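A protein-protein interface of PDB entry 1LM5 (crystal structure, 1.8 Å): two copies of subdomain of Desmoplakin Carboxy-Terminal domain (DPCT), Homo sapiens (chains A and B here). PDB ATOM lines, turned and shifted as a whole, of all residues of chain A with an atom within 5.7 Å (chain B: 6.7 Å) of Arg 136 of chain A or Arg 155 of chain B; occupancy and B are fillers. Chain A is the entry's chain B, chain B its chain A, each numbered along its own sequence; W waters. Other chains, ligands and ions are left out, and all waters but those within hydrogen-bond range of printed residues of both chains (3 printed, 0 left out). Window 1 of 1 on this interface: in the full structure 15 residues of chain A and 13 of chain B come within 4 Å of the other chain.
Thr 125 of chain A touches Gln 154 of chain B (O to CG, 3.7 Å).
Arg 151 of chain B touches Gly 126 of chain A.
Gln 154 of chain B touches Gly 126 of chain A.
His 134 of chain A touches Ser 161 of chain B.
O of Tyr 162 of chain B touches O of His 134 of chain A (3.9 Å).
CA of Gly 135 of chain A touches O of Ser 161 of chain B (2.9 Å).
C of Tyr 162 of chain B touches CA of Gly 135 of chain A (3.99 Å).
Arg 155 of chain B touches Arg 136 of chain A (CD to CB, 3.6 Å).
CA of Ile 137 of chain A touches OH of Tyr 112 of chain B, at 3.6 Å.
NH2 of Arg 155 of chain B touches CB of Ser 138 of chain A (3.3 Å).
The backbone NH of Ser 138 of chain A sits at hydrogen-bond distance from the side-chain hydroxyl of Tyr 112 of chain B (3.0 Å).
O of Arg 136 of chain A sits at hydrogen-bond distance from NE2 of Gln 116 of chain B, 3.0 Å away.
The guanidinium group (NH1) of Arg 151 of chain B is in hydrogen-bond range of the side-chain hydroxyl (OH) of Tyr 123 of chain A.
The backbone carbonyl oxygen (O) of Gly 126 of chain A sits at hydrogen-bond distance from the guanidinium group (NH1) of Arg 155 of chain B (2.7 Å).
NE of Arg 136 of chain A is in salt-bridge range of OD1 of Asp 158 of chain B, at 3.6 Å.
O of Ser 161 of chain B lies within hydrogen-bond range of N of Arg 136 of chain A.
Water W1 lies within hydrogen-bond range of OD1 of Asp 158 of chain B (2.6 Å), NH2 of Arg 136 of chain A (2.8 Å) and O of Thr 49 of chain A (3.3 Å).
Water W2 lies within hydrogen-bond range of O of Thr 125 of chain A (2.7 Å), NE2 of Gln 154 of chain B (2.7 Å) and OD1 of Asp 158 of chain B (3.3 Å).
Water W3 bridges O of Arg 136 of chain A (2.8 Å) and OE1 of Gln 116 of chain B (2.9 Å).
Hydrophobic or aromatic side chains of chain A that line the printed part of chain B: Tyr 123.
Among the printed residues, Asp or Glu carboxylates within 4 Å of a Lys or Arg side-chain nitrogen of the other chain: Arg 136 of chain A with Asp 158 of chain B (3.6 Å).
OD1 of Asp 149 of chain B sits close to N of Arg 151 of chain B (3.1 Å).
OH of Tyr 162 of chain B is in hydrogen-bond range of O of Leu 156 of chain B (2.6 Å).
The side-chain hydroxyl (OG) of Ser 160 of chain B sits at hydrogen-bond distance from the side-chain carboxylate (OD2) of Asp 158 of chain B.
The side-chain hydroxyl of Ser 161 of chain B sits at hydrogen-bond distance from the backbone carbonyl oxygen of Asp 158 of chain B, 3.0 Å away.
The backbone carbonyl oxygen (O) of Phe 121 of chain A sits at hydrogen-bond distance from the side-chain hydroxyl (OG1) of Thr 125 of chain A, at 2.7 Å.
The guanidinium group (NH1) of Arg 136 of chain A is in hydrogen-bond range of the backbone carbonyl oxygen (O) of Gln 122 of chain A, 2.8 Å away.
No position is printed for both chains.
Of the 18 pairs that touch across the chains among the printed residues, none has its exchanged pair printed and touching as well.
Of the printed residues of chain B, Thr 125 of chain A touches Gln 154.
Gly 127 of chain A touches none of the printed residues of chain B.
Arg 136 of chain A touches just these residues of chain B: Gln 116 (3.0 Å), Arg 155 (3.6 Å), Asp 158 (3.6 Å) and Ser 161 (3.2 Å).
Of the printed residues of chain A, Arg 151 of chain B touches Tyr 123 (3.0 Å) and Gly 126 (3.6 Å).
Ala 152 of chain B touches none of the printed residues of chain A.
The nearest residue of chain B that does not touch Arg 136 of chain A is Tyr 112 of chain B (4.5 Å).
The nearest residue of chain A that does not touch Arg 155 of chain B is Gly 127 of chain A (4.2 Å).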
ATOM      1  N   PRO A  10     -22.606  -8.611  20.922  1.00  0.00           N
ATOM      2  CA  PRO A  10     -22.205  -7.219  20.740  1.00  0.00           C
ATOM      3  C   PRO A  10     -22.790  -6.701  19.424  1.00  0.00           C
ATOM      4  O   PRO A  10     -23.049  -7.474  18.492  1.00  0.00           O
ATOM      5  CB  PRO A  10     -20.680  -7.295  20.654  1.00  0.00           C
ATOM      6  CG  PRO A  10     -20.334  -8.554  21.385  1.00  0.00           C
ATOM      7  CD  PRO A  10     -21.430  -9.501  20.942  1.00  0.00           C
ATOM      8  N   THR A  49     -14.263  -7.793  23.504  1.00  0.00           N
ATOM      9  CA  THR A  49     -15.027  -9.019  23.696  1.00  0.00           C
ATOM     10  C   THR A  49     -14.523 -10.139  22.795  1.00  0.00           C
ATOM     11  O   THR A  49     -15.219 -11.118  22.576  1.00  0.00           O
ATOM     12  CB  THR A  49     -16.559  -8.811  23.480  1.00  0.00           C
ATOM     13  OG1 THR A  49     -16.809  -8.218  22.198  1.00  0.00           O
ATOM     14  CG2 THR A  49     -17.128  -7.915  24.588  1.00  0.00           C
ATOM     15  N   PHE A 121     -19.019  -3.230  28.262  1.00  0.00           N
ATOM     16  CA  PHE A 121     -19.178  -3.882  26.979  1.00  0.00           C
ATOM     17  C   PHE A 121     -19.152  -5.388  27.198  1.00  0.00           C
ATOM     18  O   PHE A 121     -19.987  -6.113  26.673  1.00  0.00           O
ATOM     19  CB  PHE A 121     -18.028  -3.515  26.046  1.00  0.00           C
ATOM     20  CG  PHE A 121     -18.041  -2.088  25.585  1.00  0.00           C
ATOM     21  CD1 PHE A 121     -16.849  -1.467  25.220  1.00  0.00           C
ATOM     22  CD2 PHE A 121     -19.233  -1.381  25.473  1.00  0.00           C
ATOM     23  CE1 PHE A 121     -16.846  -0.154  24.744  1.00  0.00           C
ATOM     24  CE2 PHE A 121     -19.247  -0.065  25.000  1.00  0.00           C
ATOM     25  CZ  PHE A 121     -18.049   0.549  24.634  1.00  0.00           C
ATOM     26  N   GLN A 122     -18.173  -5.856  27.969  1.00  0.00           N
ATOM     27  CA  GLN A 122     -18.058  -7.285  28.221  1.00  0.00           C
ATOM     28  C   GLN A 122     -19.254  -7.773  29.014  1.00  0.00           C
ATOM     29  O   GLN A 122     -19.915  -8.739  28.640  1.00  0.00           O
ATOM     30  CB  GLN A 122     -16.760  -7.591  28.979  1.00  0.00           C
ATOM     31  CG  GLN A 122     -15.502  -7.238  28.195  1.00  0.00           C
ATOM     32  CD  GLN A 122     -14.226  -7.433  28.998  1.00  0.00           C
ATOM     33  OE1 GLN A 122     -14.263  -7.638  30.214  1.00  0.00           O
ATOM     34  NE2 GLN A 122     -13.085  -7.349  28.318  1.00  0.00           N
ATOM     35  N   TYR A 123     -19.537  -7.085  30.112  1.00  0.00           N
ATOM     36  CA  TYR A 123     -20.641  -7.459  30.970  1.00  0.00           C
ATOM     37  C   TYR A 123     -21.944  -7.635  30.201  1.00  0.00           C
ATOM     38  O   TYR A 123     -22.610  -8.665  30.308  1.00  0.00           O
ATOM     39  CB  TYR A 123     -20.821  -6.403  32.053  1.00  0.00           C
ATOM     40  CG  TYR A 123     -21.856  -6.796  33.065  1.00  0.00           C
ATOM     41  CD1 TYR A 123     -21.555  -7.706  34.066  1.00  0.00           C
ATOM     42  CD2 TYR A 123     -23.154  -6.287  32.998  1.00  0.00           C
ATOM     43  CE1 TYR A 123     -22.516  -8.102  34.976  1.00  0.00           C
ATOM     44  CE2 TYR A 123     -24.119  -6.678  33.904  1.00  0.00           C
ATOM     45  CZ  TYR A 123     -23.794  -7.587  34.890  1.00  0.00           C
ATOM     46  OH  TYR A 123     -24.747  -7.994  35.795  1.00  0.00           O
ATOM     47  N   THR A 125     -22.424  -8.227  27.195  1.00  0.00           N
ATOM     48  CA  THR A 125     -22.411  -9.235  26.153  1.00  0.00           C
ATOM     49  C   THR A 125     -22.089 -10.641  26.633  1.00  0.00           C
ATOM     50  O   THR A 125     -21.629 -11.476  25.858  1.00  0.00           O
ATOM     51  CB  THR A 125     -21.439  -8.842  25.034  1.00  0.00           C
ATOM     52  OG1 THR A 125     -20.141  -8.577  25.586  1.00  0.00           O
ATOM     53  CG2 THR A 125     -21.949  -7.577  24.315  1.00  0.00           C
ATOM     54  N   GLY A 126     -22.328 -10.906  27.909  1.00  0.00           N
ATOM     55  CA  GLY A 126     -22.072 -12.244  28.404  1.00  0.00           C
ATOM     56  C   GLY A 126     -21.311 -12.337  29.706  1.00  0.00           C
ATOM     57  O   GLY A 126     -21.501 -13.286  30.460  1.00  0.00           O
ATOM     58  N   GLY A 127     -20.450 -11.364  29.977  1.00  0.00           N
ATOM     59  CA  GLY A 127     -19.697 -11.407  31.210  1.00  0.00           C
ATOM     60  C   GLY A 127     -18.295 -10.897  31.006  1.00  0.00           C
ATOM     61  O   GLY A 127     -17.789 -10.874  29.886  1.00  0.00           O
ATOM     62  N   LEU A 128     -17.659 -10.500  32.099  1.00  0.00           N
ATOM     63  CA  LEU A 128     -16.312  -9.983  32.034  1.00  0.00           C
ATOM     64  C   LEU A 128     -15.369 -11.024  31.484  1.00  0.00           C
ATOM     65  O   LEU A 128     -15.570 -12.227  31.673  1.00  0.00           O
ATOM     66  CB  LEU A 128     -15.833  -9.556  33.413  1.00  0.00           C
ATOM     67  CG  LEU A 128     -16.657  -8.458  34.077  1.00  0.00           C
ATOM     68  CD1 LEU A 128     -15.919  -7.982  35.315  1.00  0.00           C
ATOM     69  CD2 LEU A 128     -16.864  -7.309  33.097  1.00  0.00           C
ATOM     70  N   VAL A 129     -14.336 -10.543  30.807  1.00  0.00           N
ATOM     71  CA  VAL A 129     -13.338 -11.408  30.213  1.00  0.00           C
ATOM     72  C   VAL A 129     -12.174 -11.644  31.158  1.00  0.00           C
ATOM     73  O   VAL A 129     -11.664 -10.711  31.774  1.00  0.00           O
ATOM     74  CB  VAL A 129     -12.773 -10.789  28.925  1.00  0.00           C
ATOM     75  CG1 VAL A 129     -11.624 -11.635  28.389  1.00  0.00           C
ATOM     76  CG2 VAL A 129     -13.876 -10.664  27.888  1.00  0.00           C
ATOM     77  N   ASP A 130     -11.777 -12.902  31.289  1.00  0.00           N
ATOM     78  CA  ASP A 130     -10.610 -13.226  32.091  1.00  0.00           C
ATOM     79  C   ASP A 130      -9.493 -13.396  31.060  1.00  0.00           C
ATOM     80  O   ASP A 130      -9.468 -14.374  30.325  1.00  0.00           O
ATOM     81  CB  ASP A 130     -10.806 -14.529  32.854  1.00  0.00           C
ATOM     82  CG  ASP A 130      -9.560 -14.937  33.598  1.00  0.00           C
ATOM     83  OD1 ASP A 130      -8.538 -14.222  33.479  1.00  0.00           O
ATOM     84  OD2 ASP A 130      -9.601 -15.963  34.299  1.00  0.00           O
ATOM     85  N   HIS A 134      -8.765 -16.017  28.325  1.00  0.00           N
ATOM     86  CA  HIS A 134      -9.453 -15.348  27.231  1.00  0.00           C
ATOM     87  C   HIS A 134     -10.877 -15.852  27.066  1.00  0.00           C
ATOM     88  O   HIS A 134     -11.336 -16.100  25.960  1.00  0.00           O
ATOM     89  CB  HIS A 134      -8.668 -15.520  25.928  1.00  0.00           C
ATOM     90  CG  HIS A 134      -7.285 -14.947  25.986  1.00  0.00           C
ATOM     91  ND1 HIS A 134      -6.196 -15.672  26.422  1.00  0.00           N
ATOM     92  CD2 HIS A 134      -6.827 -13.698  25.734  1.00  0.00           C
ATOM     93  CE1 HIS A 134      -5.128 -14.894  26.438  1.00  0.00           C
ATOM     94  NE2 HIS A 134      -5.483 -13.691  26.026  1.00  0.00           N
ATOM     95  N   GLY A 135     -11.575 -16.003  28.184  1.00  0.00           N
ATOM     96  CA  GLY A 135     -12.951 -16.455  28.133  1.00  0.00           C
ATOM     97  C   GLY A 135     -13.775 -15.552  29.020  1.00  0.00           C
ATOM     98  O   GLY A 135     -13.227 -14.723  29.739  1.00  0.00           O
ATOM     99  N   ARG A 136     -15.089 -15.696  28.969  1.00  0.00           N
ATOM    100  CA  ARG A 136     -15.946 -14.878  29.795  1.00  0.00           C
ATOM    101  C   ARG A 136     -16.233 -15.634  31.074  1.00  0.00           C
ATOM    102  O   ARG A 136     -16.275 -16.867  31.083  1.00  0.00           O
ATOM    103  CB  ARG A 136     -17.253 -14.591  29.078  1.00  0.00           C
ATOM    104  CG  ARG A 136     -17.091 -13.788  27.823  1.00  0.00           C
ATOM    105  CD  ARG A 136     -18.455 -13.579  27.226  1.00  0.00           C
ATOM    106  NE  ARG A 136     -18.434 -12.792  26.002  1.00  0.00           N
ATOM    107  CZ  ARG A 136     -18.597 -11.474  25.960  1.00  0.00           C
ATOM    108  NH1 ARG A 136     -18.779 -10.788  27.082  1.00  0.00           N
ATOM    109  NH2 ARG A 136     -18.631 -10.858  24.790  1.00  0.00           N
ATOM    110  N   ILE A 137     -16.430 -14.888  32.153  1.00  0.00           N
ATOM    111  CA  ILE A 137     -16.714 -15.497  33.432  1.00  0.00           C
ATOM    112  C   ILE A 137     -17.879 -14.795  34.086  1.00  0.00           C
ATOM    113  O   ILE A 137     -18.194 -13.649  33.755  1.00  0.00           O
ATOM    114  CB  ILE A 137     -15.495 -15.414  34.355  1.00  0.00           C
ATOM    115  CG1 ILE A 137     -15.140 -13.945  34.608  1.00  0.00           C
ATOM    116  CG2 ILE A 137     -14.342 -16.172  33.736  1.00  0.00           C
ATOM    117  CD1 ILE A 137     -14.020 -13.755  35.596  1.00  0.00           C
ATOM    118  N   SER A 138     -18.526 -15.487  35.015  1.00  0.00           N
ATOM    119  CA  SER A 138     -19.653 -14.912  35.718  1.00  0.00           C
ATOM    120  C   SER A 138     -19.097 -13.769  36.550  1.00  0.00           C
ATOM    121  O   SER A 138     -17.893 -13.702  36.809  1.00  0.00           O
ATOM    122  CB  SER A 138     -20.293 -15.952  36.645  1.00  0.00           C
ATOM    123  OG  SER A 138     -19.366 -16.354  37.645  1.00  0.00           O
ATOM    124  N   THR A 139     -19.963 -12.865  36.973  1.00  0.00           N
ATOM    125  CA  THR A 139     -19.494 -11.765  37.794  1.00  0.00           C
ATOM    126  C   THR A 139     -19.015 -12.365  39.115  1.00  0.00           C
ATOM    127  O   THR A 139     -18.018 -11.918  39.674  1.00  0.00           O
ATOM    128  CB  THR A 139     -20.605 -10.765  38.035  1.00  0.00           C
ATOM    129  OG1 THR A 139     -21.572 -11.332  38.920  1.00  0.00           O
ATOM    130  CG2 THR A 139     -21.285 -10.444  36.714  1.00  0.00           C
ATOM    131  N   GLU A 140     -19.709 -13.394  39.595  1.00  0.00           N
ATOM    132  CA  GLU A 140     -19.306 -14.044  40.834  1.00  0.00           C
ATOM    133  C   GLU A 140     -17.835 -14.451  40.725  1.00  0.00           C
ATOM    134  O   GLU A 140     -17.042 -14.208  41.635  1.00  0.00           O
ATOM    135  CB  GLU A 140     -20.150 -15.297  41.097  1.00  0.00           C
ATOM    136  CG  GLU A 140     -21.632 -15.049  41.410  1.00  0.00           C
ATOM    137  CD  GLU A 140     -22.386 -14.338  40.288  1.00  0.00           C
ATOM    138  OE1 GLU A 140     -22.244 -14.738  39.111  1.00  0.00           O
ATOM    139  OE2 GLU A 140     -23.133 -13.377  40.595  1.00  0.00           O
ATOM    140  N   TYR B 112     -15.677 -23.175  40.405  1.00  0.00           N
ATOM    141  CA  TYR B 112     -16.371 -22.553  39.289  1.00  0.00           C
ATOM    142  C   TYR B 112     -15.741 -22.993  37.977  1.00  0.00           C
ATOM    143  O   TYR B 112     -16.434 -23.430  37.059  1.00  0.00           O
ATOM    144  CB  TYR B 112     -16.288 -21.029  39.394  1.00  0.00           C
ATOM    145  CG  TYR B 112     -16.840 -20.319  38.182  1.00  0.00           C
ATOM    146  CD1 TYR B 112     -18.211 -20.116  38.033  1.00  0.00           C
ATOM    147  CD2 TYR B 112     -15.992 -19.879  37.167  1.00  0.00           C
ATOM    148  CE1 TYR B 112     -18.726 -19.490  36.898  1.00  0.00           C
ATOM    149  CE2 TYR B 112     -16.490 -19.256  36.031  1.00  0.00           C
ATOM    150  CZ  TYR B 112     -17.860 -19.064  35.903  1.00  0.00           C
ATOM    151  OH  TYR B 112     -18.365 -18.451  34.783  1.00  0.00           O
ATOM    152  N   GLN B 116     -17.903 -24.656  35.208  1.00  0.00           N
ATOM    153  CA  GLN B 116     -18.065 -23.932  33.957  1.00  0.00           C
ATOM    154  C   GLN B 116     -17.659 -24.779  32.754  1.00  0.00           C
ATOM    155  O   GLN B 116     -18.397 -24.847  31.765  1.00  0.00           O
ATOM    156  CB  GLN B 116     -17.260 -22.627  33.961  1.00  0.00           C
ATOM    157  CG  GLN B 116     -17.331 -21.890  32.624  1.00  0.00           C
ATOM    158  CD  GLN B 116     -16.525 -20.603  32.606  1.00  0.00           C
ATOM    159  OE1 GLN B 116     -15.321 -20.610  32.865  1.00  0.00           O
ATOM    160  NE2 GLN B 116     -17.188 -19.491  32.295  1.00  0.00           N
ATOM    161  N   GLU B 120     -19.951 -26.234  29.694  1.00  0.00           N
ATOM    162  CA  GLU B 120     -19.630 -25.914  28.320  1.00  0.00           C
ATOM    163  C   GLU B 120     -19.525 -27.207  27.538  1.00  0.00           C
ATOM    164  O   GLU B 120     -20.007 -27.289  26.415  1.00  0.00           O
ATOM    165  CB  GLU B 120     -18.329 -25.118  28.248  1.00  0.00           C
ATOM    166  CG  GLU B 120     -18.416 -23.838  29.072  1.00  0.00           C
ATOM    167  CD  GLU B 120     -17.164 -22.993  28.997  1.00  0.00           C
ATOM    168  OE1 GLU B 120     -16.091 -23.544  28.688  1.00  0.00           O
ATOM    169  OE2 GLU B 120     -17.255 -21.782  29.269  1.00  0.00           O
ATOM    170  N   ILE B 148     -28.154 -22.014  35.574  1.00  0.00           N
ATOM    171  CA  ILE B 148     -27.457 -20.859  35.044  1.00  0.00           C
ATOM    172  C   ILE B 148     -28.432 -19.698  35.015  1.00  0.00           C
ATOM    173  O   ILE B 148     -29.640 -19.898  35.128  1.00  0.00           O
ATOM    174  CB  ILE B 148     -27.004 -21.127  33.596  1.00  0.00           C
ATOM    175  CG1 ILE B 148     -28.193 -21.640  32.773  1.00  0.00           C
ATOM    176  CG2 ILE B 148     -25.874 -22.152  33.575  1.00  0.00           C
ATOM    177  CD1 ILE B 148     -27.918 -21.770  31.289  1.00  0.00           C
ATOM    178  N   ASP B 149     -27.917 -18.484  34.892  1.00  0.00           N
ATOM    179  CA  ASP B 149     -28.804 -17.345  34.776  1.00  0.00           C
ATOM    180  C   ASP B 149     -28.726 -16.916  33.321  1.00  0.00           C
ATOM    181  O   ASP B 149     -28.021 -17.539  32.522  1.00  0.00           O
ATOM    182  CB  ASP B 149     -28.411 -16.199  35.720  1.00  0.00           C
ATOM    183  CG  ASP B 149     -26.935 -15.826  35.647  1.00  0.00           C
ATOM    184  OD1 ASP B 149     -26.287 -16.021  34.595  1.00  0.00           O
ATOM    185  OD2 ASP B 149     -26.430 -15.301  36.663  1.00  0.00           O
ATOM    186  N   GLY B 150     -29.472 -15.882  32.963  1.00  0.00           N
ATOM    187  CA  GLY B 150     -29.462 -15.414  31.592  1.00  0.00           C
ATOM    188  C   GLY B 150     -28.065 -15.033  31.145  1.00  0.00           C
ATOM    189  O   GLY B 150     -27.714 -15.222  29.983  1.00  0.00           O
ATOM    190  N   ARG B 151     -27.278 -14.477  32.063  1.00  0.00           N
ATOM    191  CA  ARG B 151     -25.914 -14.079  31.743  1.00  0.00           C
ATOM    192  C   ARG B 151     -25.099 -15.306  31.373  1.00  0.00           C
ATOM    193  O   ARG B 151     -24.422 -15.324  30.354  1.00  0.00           O
ATOM    194  CB  ARG B 151     -25.276 -13.372  32.937  1.00  0.00           C
ATOM    195  CG  ARG B 151     -25.496 -11.882  32.934  1.00  0.00           C
ATOM    196  CD  ARG B 151     -24.550 -11.197  31.958  1.00  0.00           C
ATOM    197  NE  ARG B 151     -25.175 -10.037  31.323  1.00  0.00           N
ATOM    198  CZ  ARG B 151     -25.804  -9.067  31.978  1.00  0.00           C
ATOM    199  NH1 ARG B 151     -25.901  -9.108  33.298  1.00  0.00           N
ATOM    200  NH2 ARG B 151     -26.334  -8.052  31.311  1.00  0.00           N
ATOM    201  N   ALA B 152     -25.169 -16.330  32.211  1.00  0.00           N
ATOM    202  CA  ALA B 152     -24.432 -17.550  31.935  1.00  0.00           C
ATOM    203  C   ALA B 152     -24.936 -18.128  30.614  1.00  0.00           C
ATOM    204  O   ALA B 152     -24.163 -18.659  29.824  1.00  0.00           O
ATOM    205  CB  ALA B 152     -24.630 -18.544  33.060  1.00  0.00           C
ATOM    206  N   ALA B 153     -26.237 -18.014  30.367  1.00  0.00           N
ATOM    207  CA  ALA B 153     -26.799 -18.535  29.122  1.00  0.00           C
ATOM    208  C   ALA B 153     -26.188 -17.833  27.910  1.00  0.00           C
ATOM    209  O   ALA B 153     -25.814 -18.484  26.934  1.00  0.00           O
ATOM    210  CB  ALA B 153     -28.321 -18.374  29.119  1.00  0.00           C
ATOM    211  N   GLN B 154     -26.084 -16.508  27.971  1.00  0.00           N
ATOM    212  CA  GLN B 154     -25.503 -15.744  26.874  1.00  0.00           C
ATOM    213  C   GLN B 154     -24.054 -16.201  26.684  1.00  0.00           C
ATOM    214  O   GLN B 154     -23.591 -16.361  25.558  1.00  0.00           O
ATOM    215  CB  GLN B 154     -25.562 -14.242  27.179  1.00  0.00           C
ATOM    216  CG  GLN B 154     -24.757 -13.353  26.225  1.00  0.00           C
ATOM    217  CD  GLN B 154     -25.184 -13.474  24.771  1.00  0.00           C
ATOM    218  OE1 GLN B 154     -26.356 -13.284  24.440  1.00  0.00           O
ATOM    219  NE2 GLN B 154     -24.229 -13.781  23.891  1.00  0.00           N
ATOM    220  N   ARG B 155     -23.349 -16.409  27.793  1.00  0.00           N
ATOM    221  CA  ARG B 155     -21.961 -16.883  27.751  1.00  0.00           C
ATOM    222  C   ARG B 155     -21.891 -18.235  27.041  1.00  0.00           C
ATOM    223  O   ARG B 155     -21.107 -18.428  26.110  1.00  0.00           O
ATOM    224  CB  ARG B 155     -21.414 -17.070  29.164  1.00  0.00           C
ATOM    225  CG  ARG B 155     -20.770 -15.856  29.759  1.00  0.00           C
ATOM    226  CD  ARG B 155     -19.825 -16.253  30.880  1.00  0.00           C
ATOM    227  NE  ARG B 155     -20.503 -16.841  32.031  1.00  0.00           N
ATOM    228  CZ  ARG B 155     -21.354 -16.184  32.814  1.00  0.00           C
ATOM    229  NH1 ARG B 155     -21.644 -14.911  32.572  1.00  0.00           N
ATOM    230  NH2 ARG B 155     -21.903 -16.798  33.850  1.00  0.00           N
ATOM    231  N   LEU B 156     -22.702 -19.177  27.509  1.00  0.00           N
ATOM    232  CA  LEU B 156     -22.734 -20.517  26.932  1.00  0.00           C
ATOM    233  C   LEU B 156     -23.091 -20.521  25.459  1.00  0.00           C
ATOM    234  O   LEU B 156     -22.489 -21.243  24.663  1.00  0.00           O
ATOM    235  CB  LEU B 156     -23.736 -21.402  27.672  1.00  0.00           C
ATOM    236  CG  LEU B 156     -23.306 -21.860  29.058  1.00  0.00           C
ATOM    237  CD1 LEU B 156     -24.450 -22.605  29.703  1.00  0.00           C
ATOM    238  CD2 LEU B 156     -22.070 -22.750  28.944  1.00  0.00           C
ATOM    239  N   GLN B 157     -24.079 -19.716  25.093  1.00  0.00           N
ATOM    240  CA  GLN B 157     -24.512 -19.666  23.709  1.00  0.00           C
ATOM    241  C   GLN B 157     -23.443 -19.085  22.812  1.00  0.00           C
ATOM    242  O   GLN B 157     -23.336 -19.469  21.646  1.00  0.00           O
ATOM    243  CB  GLN B 157     -25.806 -18.865  23.601  1.00  0.00           C
ATOM    244  CG  GLN B 157     -26.988 -19.597  24.190  1.00  0.00           C
ATOM    245  CD  GLN B 157     -28.192 -18.699  24.362  1.00  0.00           C
ATOM    246  OE1 GLN B 157     -28.508 -17.900  23.480  1.00  0.00           O
ATOM    247  NE2 GLN B 157     -28.872 -18.827  25.495  1.00  0.00           N
ATOM    248  N   ASP B 158     -22.652 -18.172  23.367  1.00  0.00           N
ATOM    249  CA  ASP B 158     -21.564 -17.528  22.648  1.00  0.00           C
ATOM    250  C   ASP B 158     -20.328 -18.416  22.748  1.00  0.00           C
ATOM    251  O   ASP B 158     -19.363 -18.079  23.432  1.00  0.00           O
ATOM    252  CB  ASP B 158     -21.242 -16.174  23.267  1.00  0.00           C
ATOM    253  CG  ASP B 158     -20.130 -15.457  22.537  1.00  0.00           C
ATOM    254  OD1 ASP B 158     -19.639 -14.429  23.053  1.00  0.00           O
ATOM    255  OD2 ASP B 158     -19.746 -15.926  21.443  1.00  0.00           O
ATOM    256  N   THR B 159     -20.366 -19.542  22.052  1.00  0.00           N
ATOM    257  CA  THR B 159     -19.262 -20.492  22.087  1.00  0.00           C
ATOM    258  C   THR B 159     -17.913 -19.896  21.693  1.00  0.00           C
ATOM    259  O   THR B 159     -16.865 -20.470  21.991  1.00  0.00           O
ATOM    260  CB  THR B 159     -19.570 -21.703  21.190  1.00  0.00           C
ATOM    261  OG1 THR B 159     -19.811 -21.262  19.848  1.00  0.00           O
ATOM    262  CG2 THR B 159     -20.797 -22.440  21.706  1.00  0.00           C
ATOM    263  N   SER B 160     -17.926 -18.736  21.042  1.00  0.00           N
ATOM    264  CA  SER B 160     -16.684 -18.108  20.619  1.00  0.00           C
ATOM    265  C   SER B 160     -15.885 -17.533  21.775  1.00  0.00           C
ATOM    266  O   SER B 160     -14.698 -17.252  21.636  1.00  0.00           O
ATOM    267  CB  SER B 160     -16.964 -16.993  19.603  1.00  0.00           C
ATOM    268  OG  SER B 160     -17.576 -15.864  20.213  1.00  0.00           O
ATOM    269  N   SER B 161     -16.519 -17.359  22.922  1.00  0.00           N
ATOM    270  CA  SER B 161     -15.809 -16.775  24.045  1.00  0.00           C
ATOM    271  C   SER B 161     -15.462 -17.742  25.154  1.00  0.00           C
ATOM    272  O   SER B 161     -14.997 -17.318  26.209  1.00  0.00           O
ATOM    273  CB  SER B 161     -16.605 -15.594  24.611  1.00  0.00           C
ATOM    274  OG  SER B 161     -17.929 -15.982  24.936  1.00  0.00           O
ATOM    275  N   TYR B 162     -15.679 -19.037  24.931  1.00  0.00           N
ATOM    276  CA  TYR B 162     -15.329 -20.018  25.955  1.00  0.00           C
ATOM    277  C   TYR B 162     -13.862 -19.913  26.356  1.00  0.00           C
ATOM    278  O   TYR B 162     -12.999 -19.634  25.532  1.00  0.00           O
ATOM    279  CB  TYR B 162     -15.576 -21.444  25.465  1.00  0.00           C
ATOM    280  CG  TYR B 162     -17.013 -21.878  25.459  1.00  0.00           C
ATOM    281  CD1 TYR B 162     -17.340 -23.222  25.262  1.00  0.00           C
ATOM    282  CD2 TYR B 162     -18.055 -20.960  25.633  1.00  0.00           C
ATOM    283  CE1 TYR B 162     -18.652 -23.645  25.239  1.00  0.00           C
ATOM    284  CE2 TYR B 162     -19.384 -21.377  25.611  1.00  0.00           C
ATOM    285  CZ  TYR B 162     -19.670 -22.730  25.413  1.00  0.00           C
ATOM    286  OH  TYR B 162     -20.965 -23.180  25.406  1.00  0.00           O
ATOM    287  N   ALA B 163     -13.591 -20.154  27.631  1.00  0.00           N
ATOM    288  CA  ALA B 163     -12.238 -20.110  28.153  1.00  0.00           C
ATOM    289  C   ALA B 163     -11.348 -21.048  27.330  1.00  0.00           C
ATOM    290  O   ALA B 163     -11.773 -22.138  26.955  1.00  0.00           O
ATOM    291  CB  ALA B 163     -12.247 -20.538  29.609  1.00  0.00           C
HETATM  292  O   HOH W   1     -18.303 -12.255  22.396  1.00  0.00           O
HETATM  293  O   HOH W   2     -22.078 -12.189  23.287  1.00  0.00           O
HETATM  294  O   HOH W   3     -14.088 -18.574  31.146  1.00  0.00           O
